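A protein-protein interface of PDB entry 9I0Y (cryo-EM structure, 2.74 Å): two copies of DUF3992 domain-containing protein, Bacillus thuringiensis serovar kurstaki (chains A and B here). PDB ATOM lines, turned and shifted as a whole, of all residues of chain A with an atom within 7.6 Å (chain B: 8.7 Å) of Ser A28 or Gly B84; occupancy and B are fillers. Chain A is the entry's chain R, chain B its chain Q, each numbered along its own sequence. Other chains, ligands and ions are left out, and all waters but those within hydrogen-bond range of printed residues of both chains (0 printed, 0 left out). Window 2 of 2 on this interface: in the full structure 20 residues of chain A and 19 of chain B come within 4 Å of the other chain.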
ATOM      1  N   SER A  25      34.882 -10.073   1.009  1.00  0.00           N
ATOM      2  CA  SER A  25      33.599  -9.462   0.699  1.00  0.00           C
ATOM      3  C   SER A  25      33.540  -9.100  -0.777  1.00  0.00           C
ATOM      4  O   SER A  25      34.555  -8.704  -1.362  1.00  0.00           O
ATOM      5  CB  SER A  25      33.354  -8.210   1.554  1.00  0.00           C
ATOM      6  OG  SER A  25      34.166  -7.130   1.130  1.00  0.00           O
ATOM      7  N   PRO A  26      32.377  -9.238  -1.406  1.00  0.00           N
ATOM      8  CA  PRO A  26      32.194  -8.717  -2.761  1.00  0.00           C
ATOM      9  C   PRO A  26      31.851  -7.234  -2.742  1.00  0.00           C
ATOM     10  O   PRO A  26      31.312  -6.703  -1.769  1.00  0.00           O
ATOM     11  CB  PRO A  26      31.017  -9.546  -3.290  1.00  0.00           C
ATOM     12  CG  PRO A  26      30.210  -9.826  -2.072  1.00  0.00           C
ATOM     13  CD  PRO A  26      31.187  -9.966  -0.930  1.00  0.00           C
ATOM     14  N   TRP A  27      32.178  -6.567  -3.844  1.00  0.00           N
ATOM     15  CA  TRP A  27      31.932  -5.140  -3.971  1.00  0.00           C
ATOM     16  C   TRP A  27      31.279  -4.847  -5.312  1.00  0.00           C
ATOM     17  O   TRP A  27      31.515  -5.539  -6.307  1.00  0.00           O
ATOM     18  CB  TRP A  27      33.224  -4.322  -3.822  1.00  0.00           C
ATOM     19  CG  TRP A  27      34.274  -4.609  -4.851  1.00  0.00           C
ATOM     20  CD1 TRP A  27      35.292  -5.507  -4.751  1.00  0.00           C
ATOM     21  CD2 TRP A  27      34.419  -3.978  -6.129  1.00  0.00           C
ATOM     22  NE1 TRP A  27      36.059  -5.484  -5.889  1.00  0.00           N
ATOM     23  CE2 TRP A  27      35.543  -4.553  -6.751  1.00  0.00           C
ATOM     24  CE3 TRP A  27      33.707  -2.988  -6.810  1.00  0.00           C
ATOM     25  CZ2 TRP A  27      35.970  -4.171  -8.020  1.00  0.00           C
ATOM     26  CZ3 TRP A  27      34.131  -2.611  -8.066  1.00  0.00           C
ATOM     27  CH2 TRP A  27      35.252  -3.201  -8.659  1.00  0.00           C
ATOM     28  N   SER A  28      30.447  -3.809  -5.321  1.00  0.00           N
ATOM     29  CA  SER A  28      29.737  -3.376  -6.513  1.00  0.00           C
ATOM     30  C   SER A  28      29.602  -1.861  -6.483  1.00  0.00           C
ATOM     31  O   SER A  28      29.635  -1.233  -5.422  1.00  0.00           O
ATOM     32  CB  SER A  28      28.359  -4.040  -6.615  1.00  0.00           C
ATOM     33  OG  SER A  28      27.541  -3.374  -7.556  1.00  0.00           O
ATOM     34  N   GLY A  29      29.457  -1.277  -7.668  1.00  0.00           N
ATOM     35  CA  GLY A  29      29.286   0.158  -7.785  1.00  0.00           C
ATOM     36  C   GLY A  29      28.720   0.585  -9.123  1.00  0.00           C
ATOM     37  O   GLY A  29      29.216   0.169 -10.170  1.00  0.00           O
ATOM     38  N   THR A  30      27.687   1.424  -9.106  1.00  0.00           N
ATOM     39  CA  THR A  30      27.021   1.874 -10.324  1.00  0.00           C
ATOM     40  C   THR A  30      27.365   3.339 -10.562  1.00  0.00           C
ATOM     41  O   THR A  30      27.018   4.206  -9.754  1.00  0.00           O
ATOM     42  CB  THR A  30      25.511   1.676 -10.226  1.00  0.00           C
ATOM     43  OG1 THR A  30      25.229   0.336  -9.807  1.00  0.00           O
ATOM     44  CG2 THR A  30      24.857   1.926 -11.573  1.00  0.00           C
ATOM     45  N   ILE A  36      33.187   7.508  -8.528  1.00  0.00           N
ATOM     46  CA  ILE A  36      32.935   6.831  -7.261  1.00  0.00           C
ATOM     47  C   ILE A  36      34.273   6.467  -6.625  1.00  0.00           C
ATOM     48  O   ILE A  36      35.249   6.156  -7.308  1.00  0.00           O
ATOM     49  CB  ILE A  36      32.041   5.586  -7.441  1.00  0.00           C
ATOM     50  CG1 ILE A  36      30.703   5.987  -8.065  1.00  0.00           C
ATOM     51  CG2 ILE A  36      31.800   4.881  -6.115  1.00  0.00           C
ATOM     52  CD1 ILE A  36      29.579   4.999  -7.824  1.00  0.00           C
ATOM     53  N   ASN A  38      34.727   4.046  -4.039  1.00  0.00           N
ATOM     54  CA  ASN A  38      34.198   2.952  -3.229  1.00  0.00           C
ATOM     55  C   ASN A  38      35.249   2.377  -2.286  1.00  0.00           C
ATOM     56  O   ASN A  38      36.217   1.756  -2.728  1.00  0.00           O
ATOM     57  CB  ASN A  38      33.658   1.851  -4.144  1.00  0.00           C
ATOM     58  CG  ASN A  38      32.442   1.159  -3.571  1.00  0.00           C
ATOM     59  OD1 ASN A  38      32.527   0.035  -3.080  1.00  0.00           O
ATOM     60  ND2 ASN A  38      31.297   1.827  -3.634  1.00  0.00           N
ATOM     61  N   LEU A  40      36.672  -0.253   0.273  1.00  0.00           N
ATOM     62  CA  LEU A  40      36.476  -1.670   0.541  1.00  0.00           C
ATOM     63  C   LEU A  40      36.867  -2.080   1.951  1.00  0.00           C
ATOM     64  O   LEU A  40      36.317  -3.054   2.471  1.00  0.00           O
ATOM     65  CB  LEU A  40      37.277  -2.519  -0.453  1.00  0.00           C
ATOM     66  CG  LEU A  40      37.281  -2.090  -1.920  1.00  0.00           C
ATOM     67  CD1 LEU A  40      38.305  -2.891  -2.698  1.00  0.00           C
ATOM     68  CD2 LEU A  40      35.905  -2.248  -2.530  1.00  0.00           C
ATOM     69  N   VAL A  99      38.591   1.628  -4.328  1.00  0.00           N
ATOM     70  CA  VAL A  99      38.593   1.564  -5.784  1.00  0.00           C
ATOM     71  C   VAL A  99      37.945   2.837  -6.314  1.00  0.00           C
ATOM     72  O   VAL A  99      36.842   3.214  -5.897  1.00  0.00           O
ATOM     73  CB  VAL A  99      37.885   0.303  -6.309  1.00  0.00           C
ATOM     74  CG1 VAL A  99      38.656  -0.940  -5.905  1.00  0.00           C
ATOM     75  CG2 VAL A  99      36.461   0.213  -5.795  1.00  0.00           C
ATOM     76  N   LEU A 101      36.337   4.592  -9.484  1.00  0.00           N
ATOM     77  CA  LEU A 101      35.569   4.348 -10.695  1.00  0.00           C
ATOM     78  C   LEU A 101      35.331   5.663 -11.425  1.00  0.00           C
ATOM     79  O   LEU A 101      34.674   6.561 -10.880  1.00  0.00           O
ATOM     80  CB  LEU A 101      34.229   3.699 -10.361  1.00  0.00           C
ATOM     81  CG  LEU A 101      34.229   2.606  -9.292  1.00  0.00           C
ATOM     82  CD1 LEU A 101      32.825   2.080  -9.065  1.00  0.00           C
ATOM     83  CD2 LEU A 101      35.164   1.476  -9.673  1.00  0.00           C
ATOM     84  N   THR A 108      27.893  -0.673 -14.322  1.00  0.00           N
ATOM     85  CA  THR A 108      28.074  -1.363 -13.052  1.00  0.00           C
ATOM     86  C   THR A 108      29.416  -2.085 -13.030  1.00  0.00           C
ATOM     87  O   THR A 108      29.745  -2.831 -13.956  1.00  0.00           O
ATOM     88  CB  THR A 108      26.941  -2.361 -12.811  1.00  0.00           C
ATOM     89  OG1 THR A 108      25.680  -1.686 -12.905  1.00  0.00           O
ATOM     90  CG2 THR A 108      27.069  -2.992 -11.434  1.00  0.00           C
ATOM     91  N   TYR A 109      30.181  -1.855 -11.969  1.00  0.00           N
ATOM     92  CA  TYR A 109      31.442  -2.537 -11.722  1.00  0.00           C
ATOM     93  C   TYR A 109      31.255  -3.497 -10.557  1.00  0.00           C
ATOM     94  O   TYR A 109      30.694  -3.128  -9.524  1.00  0.00           O
ATOM     95  CB  TYR A 109      32.560  -1.541 -11.398  1.00  0.00           C
ATOM     96  CG  TYR A 109      32.722  -0.415 -12.394  1.00  0.00           C
ATOM     97  CD1 TYR A 109      31.856   0.670 -12.398  1.00  0.00           C
ATOM     98  CD2 TYR A 109      33.748  -0.431 -13.323  1.00  0.00           C
ATOM     99  CE1 TYR A 109      32.006   1.700 -13.304  1.00  0.00           C
ATOM    100  CE2 TYR A 109      33.908   0.594 -14.232  1.00  0.00           C
ATOM    101  CZ  TYR A 109      33.034   1.656 -14.219  1.00  0.00           C
ATOM    102  OH  TYR A 109      33.190   2.678 -15.124  1.00  0.00           O
ATOM    103  N   GLN A 110      31.720  -4.732 -10.728  1.00  0.00           N
ATOM    104  CA  GLN A 110      31.566  -5.755  -9.706  1.00  0.00           C
ATOM    105  C   GLN A 110      32.882  -6.496  -9.527  1.00  0.00           C
ATOM    106  O   GLN A 110      33.665  -6.648 -10.467  1.00  0.00           O
ATOM    107  CB  GLN A 110      30.445  -6.737 -10.062  1.00  0.00           C
ATOM    108  CG  GLN A 110      29.096  -6.366  -9.479  1.00  0.00           C
ATOM    109  CD  GLN A 110      27.943  -6.955 -10.260  1.00  0.00           C
ATOM    110  OE1 GLN A 110      27.957  -6.971 -11.489  1.00  0.00           O
ATOM    111  NE2 GLN A 110      26.935  -7.443  -9.549  1.00  0.00           N
ATOM    112  N   GLY A 111      33.118  -6.959  -8.307  1.00  0.00           N
ATOM    113  CA  GLY A 111      34.340  -7.684  -8.024  1.00  0.00           C
ATOM    114  C   GLY A 111      34.350  -8.231  -6.616  1.00  0.00           C
ATOM    115  O   GLY A 111      33.335  -8.211  -5.919  1.00  0.00           O
ATOM    116  N   GLU A 112      35.523  -8.702  -6.199  1.00  0.00           N
ATOM    117  CA  GLU A 112      35.697  -9.323  -4.892  1.00  0.00           C
ATOM    118  C   GLU A 112      36.928  -8.745  -4.209  1.00  0.00           C
ATOM    119  O   GLU A 112      37.786  -8.132  -4.844  1.00  0.00           O
ATOM    120  CB  GLU A 112      35.818 -10.846  -5.011  1.00  0.00           C
ATOM    121  CG  GLU A 112      35.204 -11.604  -3.850  1.00  0.00           C
ATOM    122  CD  GLU A 112      35.895 -12.926  -3.589  1.00  0.00           C
ATOM    123  OE1 GLU A 112      36.057 -13.288  -2.404  1.00  0.00           O
ATOM    124  OE2 GLU A 112      36.272 -13.604  -4.568  1.00  0.00           O
ATOM    125  N   VAL B  55      29.885  -5.310   7.011  1.00  0.00           N
ATOM    126  CA  VAL B  55      28.480  -4.929   6.937  1.00  0.00           C
ATOM    127  C   VAL B  55      28.077  -4.966   5.469  1.00  0.00           C
ATOM    128  O   VAL B  55      28.732  -4.340   4.628  1.00  0.00           O
ATOM    129  CB  VAL B  55      28.228  -3.534   7.533  1.00  0.00           C
ATOM    130  CG1 VAL B  55      26.764  -3.156   7.402  1.00  0.00           C
ATOM    131  CG2 VAL B  55      28.667  -3.489   8.985  1.00  0.00           C
ATOM    132  N   ARG B  56      27.010  -5.699   5.161  1.00  0.00           N
ATOM    133  CA  ARG B  56      26.524  -5.865   3.798  1.00  0.00           C
ATOM    134  C   ARG B  56      25.195  -5.142   3.637  1.00  0.00           C
ATOM    135  O   ARG B  56      24.246  -5.414   4.375  1.00  0.00           O
ATOM    136  CB  ARG B  56      26.352  -7.344   3.451  1.00  0.00           C
ATOM    137  CG  ARG B  56      27.338  -7.868   2.428  1.00  0.00           C
ATOM    138  CD  ARG B  56      27.428  -9.383   2.465  1.00  0.00           C
ATOM    139  NE  ARG B  56      28.809  -9.852   2.455  1.00  0.00           N
ATOM    140  CZ  ARG B  56      29.173 -11.110   2.660  1.00  0.00           C
ATOM    141  NH1 ARG B  56      28.282 -12.057   2.900  1.00  0.00           N
ATOM    142  NH2 ARG B  56      30.464 -11.425   2.623  1.00  0.00           N
ATOM    143  N   TYR B  57      25.134  -4.236   2.663  1.00  0.00           N
ATOM    144  CA  TYR B  57      23.918  -3.519   2.303  1.00  0.00           C
ATOM    145  C   TYR B  57      23.356  -4.164   1.041  1.00  0.00           C
ATOM    146  O   TYR B  57      23.950  -4.055  -0.037  1.00  0.00           O
ATOM    147  CB  TYR B  57      24.231  -2.039   2.088  1.00  0.00           C
ATOM    148  CG  TYR B  57      23.046  -1.136   1.839  1.00  0.00           C
ATOM    149  CD1 TYR B  57      21.744  -1.576   2.029  1.00  0.00           C
ATOM    150  CD2 TYR B  57      23.237   0.170   1.416  1.00  0.00           C
ATOM    151  CE1 TYR B  57      20.670  -0.739   1.797  1.00  0.00           C
ATOM    152  CE2 TYR B  57      22.176   1.008   1.184  1.00  0.00           C
ATOM    153  CZ  TYR B  57      20.896   0.553   1.375  1.00  0.00           C
ATOM    154  OH  TYR B  57      19.845   1.401   1.139  1.00  0.00           O
ATOM    155  N   ASP B  58      22.216  -4.843   1.181  1.00  0.00           N
ATOM    156  CA  ASP B  58      21.645  -5.628   0.091  1.00  0.00           C
ATOM    157  C   ASP B  58      20.600  -4.854  -0.703  1.00  0.00           C
ATOM    158  O   ASP B  58      20.758  -4.649  -1.909  1.00  0.00           O
ATOM    159  CB  ASP B  58      21.034  -6.920   0.636  1.00  0.00           C
ATOM    160  CG  ASP B  58      22.071  -7.851   1.232  1.00  0.00           C
ATOM    161  OD1 ASP B  58      23.272  -7.667   0.944  1.00  0.00           O
ATOM    162  OD2 ASP B  58      21.688  -8.769   1.989  1.00  0.00           O
ATOM    163  N   VAL B  59      19.526  -4.423  -0.044  1.00  0.00           N
ATOM    164  CA  VAL B  59      18.428  -3.723  -0.702  1.00  0.00           C
ATOM    165  C   VAL B  59      18.056  -2.499   0.122  1.00  0.00           C
ATOM    166  O   VAL B  59      18.084  -2.531   1.357  1.00  0.00           O
ATOM    167  CB  VAL B  59      17.203  -4.638  -0.908  1.00  0.00           C
ATOM    168  CG1 VAL B  59      17.486  -5.680  -1.977  1.00  0.00           C
ATOM    169  CG2 VAL B  59      16.812  -5.308   0.395  1.00  0.00           C
ATOM    170  N   GLY B  60      17.716  -1.415  -0.567  1.00  0.00           N
ATOM    171  CA  GLY B  60      17.327  -0.189   0.088  1.00  0.00           C
ATOM    172  C   GLY B  60      17.101   0.948  -0.884  1.00  0.00           C
ATOM    173  O   GLY B  60      17.708   1.014  -1.957  1.00  0.00           O
ATOM    174  N   ALA B  62      17.990   4.090  -0.712  1.00  0.00           N
ATOM    175  CA  ALA B  62      18.993   5.142  -0.816  1.00  0.00           C
ATOM    176  C   ALA B  62      20.282   4.761  -0.094  1.00  0.00           C
ATOM    177  O   ALA B  62      20.307   3.769   0.645  1.00  0.00           O
ATOM    178  CB  ALA B  62      18.432   6.448  -0.248  1.00  0.00           C
ATOM    179  N   ILE B  64      23.111   4.592   2.734  1.00  0.00           N
ATOM    180  CA  ILE B  64      23.053   4.604   4.189  1.00  0.00           C
ATOM    181  C   ILE B  64      24.440   4.946   4.717  1.00  0.00           C
ATOM    182  O   ILE B  64      25.424   4.960   3.975  1.00  0.00           O
ATOM    183  CB  ILE B  64      22.575   3.256   4.760  1.00  0.00           C
ATOM    184  CG1 ILE B  64      23.592   2.158   4.446  1.00  0.00           C
ATOM    185  CG2 ILE B  64      21.225   2.891   4.184  1.00  0.00           C
ATOM    186  CD1 ILE B  64      23.572   1.007   5.419  1.00  0.00           C
ATOM    187  N   LEU B  81      27.450   3.783   2.246  1.00  0.00           N
ATOM    188  CA  LEU B  81      27.196   2.561   1.497  1.00  0.00           C
ATOM    189  C   LEU B  81      26.015   2.756   0.560  1.00  0.00           C
ATOM    190  O   LEU B  81      25.042   3.432   0.902  1.00  0.00           O
ATOM    191  CB  LEU B  81      26.921   1.381   2.436  1.00  0.00           C
ATOM    192  CG  LEU B  81      28.035   0.347   2.581  1.00  0.00           C
ATOM    193  CD1 LEU B  81      29.293   1.000   3.116  1.00  0.00           C
ATOM    194  CD2 LEU B  81      27.592  -0.793   3.479  1.00  0.00           C
ATOM    195  N   ASN B  82      26.107   2.150  -0.620  1.00  0.00           N
ATOM    196  CA  ASN B  82      25.054   2.097  -1.618  1.00  0.00           C
ATOM    197  C   ASN B  82      24.487   0.683  -1.701  1.00  0.00           C
ATOM    198  O   ASN B  82      25.176  -0.282  -1.360  1.00  0.00           O
ATOM    199  CB  ASN B  82      25.580   2.524  -2.994  1.00  0.00           C
ATOM    200  CG  ASN B  82      25.775   4.022  -3.102  1.00  0.00           C
ATOM    201  OD1 ASN B  82      26.770   4.567  -2.624  1.00  0.00           O
ATOM    202  ND2 ASN B  82      24.820   4.698  -3.728  1.00  0.00           N
ATOM    203  N   PRO B  83      23.235   0.522  -2.125  1.00  0.00           N
ATOM    204  CA  PRO B  83      22.618  -0.811  -2.107  1.00  0.00           C
ATOM    205  C   PRO B  83      23.399  -1.820  -2.937  1.00  0.00           C
ATOM    206  O   PRO B  83      23.861  -1.522  -4.041  1.00  0.00           O
ATOM    207  CB  PRO B  83      21.225  -0.558  -2.692  1.00  0.00           C
ATOM    208  CG  PRO B  83      20.956   0.874  -2.413  1.00  0.00           C
ATOM    209  CD  PRO B  83      22.277   1.565  -2.529  1.00  0.00           C
ATOM    210  N   GLY B  84      23.542  -3.026  -2.393  1.00  0.00           N
ATOM    211  CA  GLY B  84      24.198  -4.117  -3.085  1.00  0.00           C
ATOM    212  C   GLY B  84      25.690  -4.236  -2.867  1.00  0.00           C
ATOM    213  O   GLY B  84      26.352  -4.926  -3.650  1.00  0.00           O
ATOM    214  N   THR B  85      26.246  -3.599  -1.840  1.00  0.00           N
ATOM    215  CA  THR B  85      27.689  -3.611  -1.623  1.00  0.00           C
ATOM    216  C   THR B  85      28.004  -4.081  -0.206  1.00  0.00           C
ATOM    217  O   THR B  85      27.115  -4.442   0.568  1.00  0.00           O
ATOM    218  CB  THR B  85      28.299  -2.230  -1.891  1.00  0.00           C
ATOM    219  OG1 THR B  85      29.712  -2.363  -2.093  1.00  0.00           O
ATOM    220  CG2 THR B  85      28.049  -1.290  -0.725  1.00  0.00           C
ATOM    221  N   SER B  86      29.293  -4.087   0.126  1.00  0.00           N
ATOM    222  CA  SER B  86      29.775  -4.525   1.427  1.00  0.00           C
ATOM    223  C   SER B  86      30.924  -3.625   1.865  1.00  0.00           C
ATOM    224  O   SER B  86      31.599  -2.998   1.045  1.00  0.00           O
ATOM    225  CB  SER B  86      30.218  -5.992   1.384  1.00  0.00           C
ATOM    226  OG  SER B  86      30.703  -6.418   2.644  1.00  0.00           O
ATOM    227  N   ILE B  87      31.142  -3.557   3.177  1.00  0.00           N
ATOM    228  CA  ILE B  87      32.273  -2.821   3.733  1.00  0.00           C
ATOM    229  C   ILE B  87      32.913  -3.661   4.830  1.00  0.00           C
ATOM    230  O   ILE B  87      32.225  -4.165   5.722  1.00  0.00           O
ATOM    231  CB  ILE B  87      31.852  -1.435   4.262  1.00  0.00           C
ATOM    232  CG1 ILE B  87      33.042  -0.708   4.890  1.00  0.00           C
ATOM    233  CG2 ILE B  87      30.710  -1.553   5.259  1.00  0.00           C
ATOM    234  CD1 ILE B  87      33.974  -0.081   3.887  1.00  0.00           C
ATOM    235  N   GLN B 110      17.561  -3.440   4.136  1.00  0.00           N
ATOM    236  CA  GLN B 110      17.881  -4.770   4.627  1.00  0.00           C
ATOM    237  C   GLN B 110      19.337  -5.087   4.325  1.00  0.00           C
ATOM    238  O   GLN B 110      19.901  -4.622   3.333  1.00  0.00           O
ATOM    239  CB  GLN B 110      16.965  -5.831   4.005  1.00  0.00           C
ATOM    240  CG  GLN B 110      15.733  -6.141   4.833  1.00  0.00           C
ATOM    241  CD  GLN B 110      14.602  -6.704   4.003  1.00  0.00           C
ATOM    242  OE1 GLN B 110      14.343  -6.243   2.894  1.00  0.00           O
ATOM    243  NE2 GLN B 110      13.920  -7.708   4.539  1.00  0.00           N
ATOM    244  N   GLY B 111      19.942  -5.888   5.193  1.00  0.00           N
ATOM    245  CA  GLY B 111      21.329  -6.257   5.003  1.00  0.00           C
ATOM    246  C   GLY B 111      21.780  -7.272   6.027  1.00  0.00           C
ATOM    247  O   GLY B 111      20.973  -7.828   6.770  1.00  0.00           O
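O of Val B55 lies close to OG of Ser B86 (3.5 Å). The backbone carbonyl oxygen (O) of Tyr B57 sits at hydrogen-bond distance from the backbone NH (N) of Gly B84, at 2.6 Å. The backbone NH (N) of Tyr B57 sits at hydrogen-bond distance from the backbone carbonyl oxygen (O) of Thr B85, 2.9 Å away. O of Asp B58 sits at hydrogen-bond distance from N of Gly B84, at 3.3 Å. The backbone NH (N) of Val A99 lies within hydrogen-bond range of the backbone carbonyl oxygen (O) of Asn A38 (2.9 Å).
Among the printed residues, merely in contact across the chains: Ser A25 with Ser B86 (3.4 Å), Pro A26 with Arg B56 (3.9 Å), Pro A26 with Ser B86 (3.4 Å), Ser A28 with Gly B84 (3.7 Å), Ser A28 with Thr B85 (3.5 Å) and Asn A38 with Thr B85 (3.8 Å).
Of the printed residues of chain B, Ser A25 touches Ser B86. Of the printed residues of chain B, Pro A26 touches Arg B56 and Ser B86. Ser A28 touches two residues of chain B. No residue of chain B comes within 4 Å of Gly A29. Tyr A109 touches none of the printed residues of chain B. Gly B84 touches just one residue of chain A: Ser A28. The nearest residue of chain A that does not touch Gly B84 is Trp A27 (5.2 Å).
Of the 16 printed residues of chain A, 4 touch a printed residue of chain B. Hydrophobic or aromatic side chains of chain A within 4 Å of the printed part of chain B: Pro A26.
Positions printed for both chains: 110 and 111.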
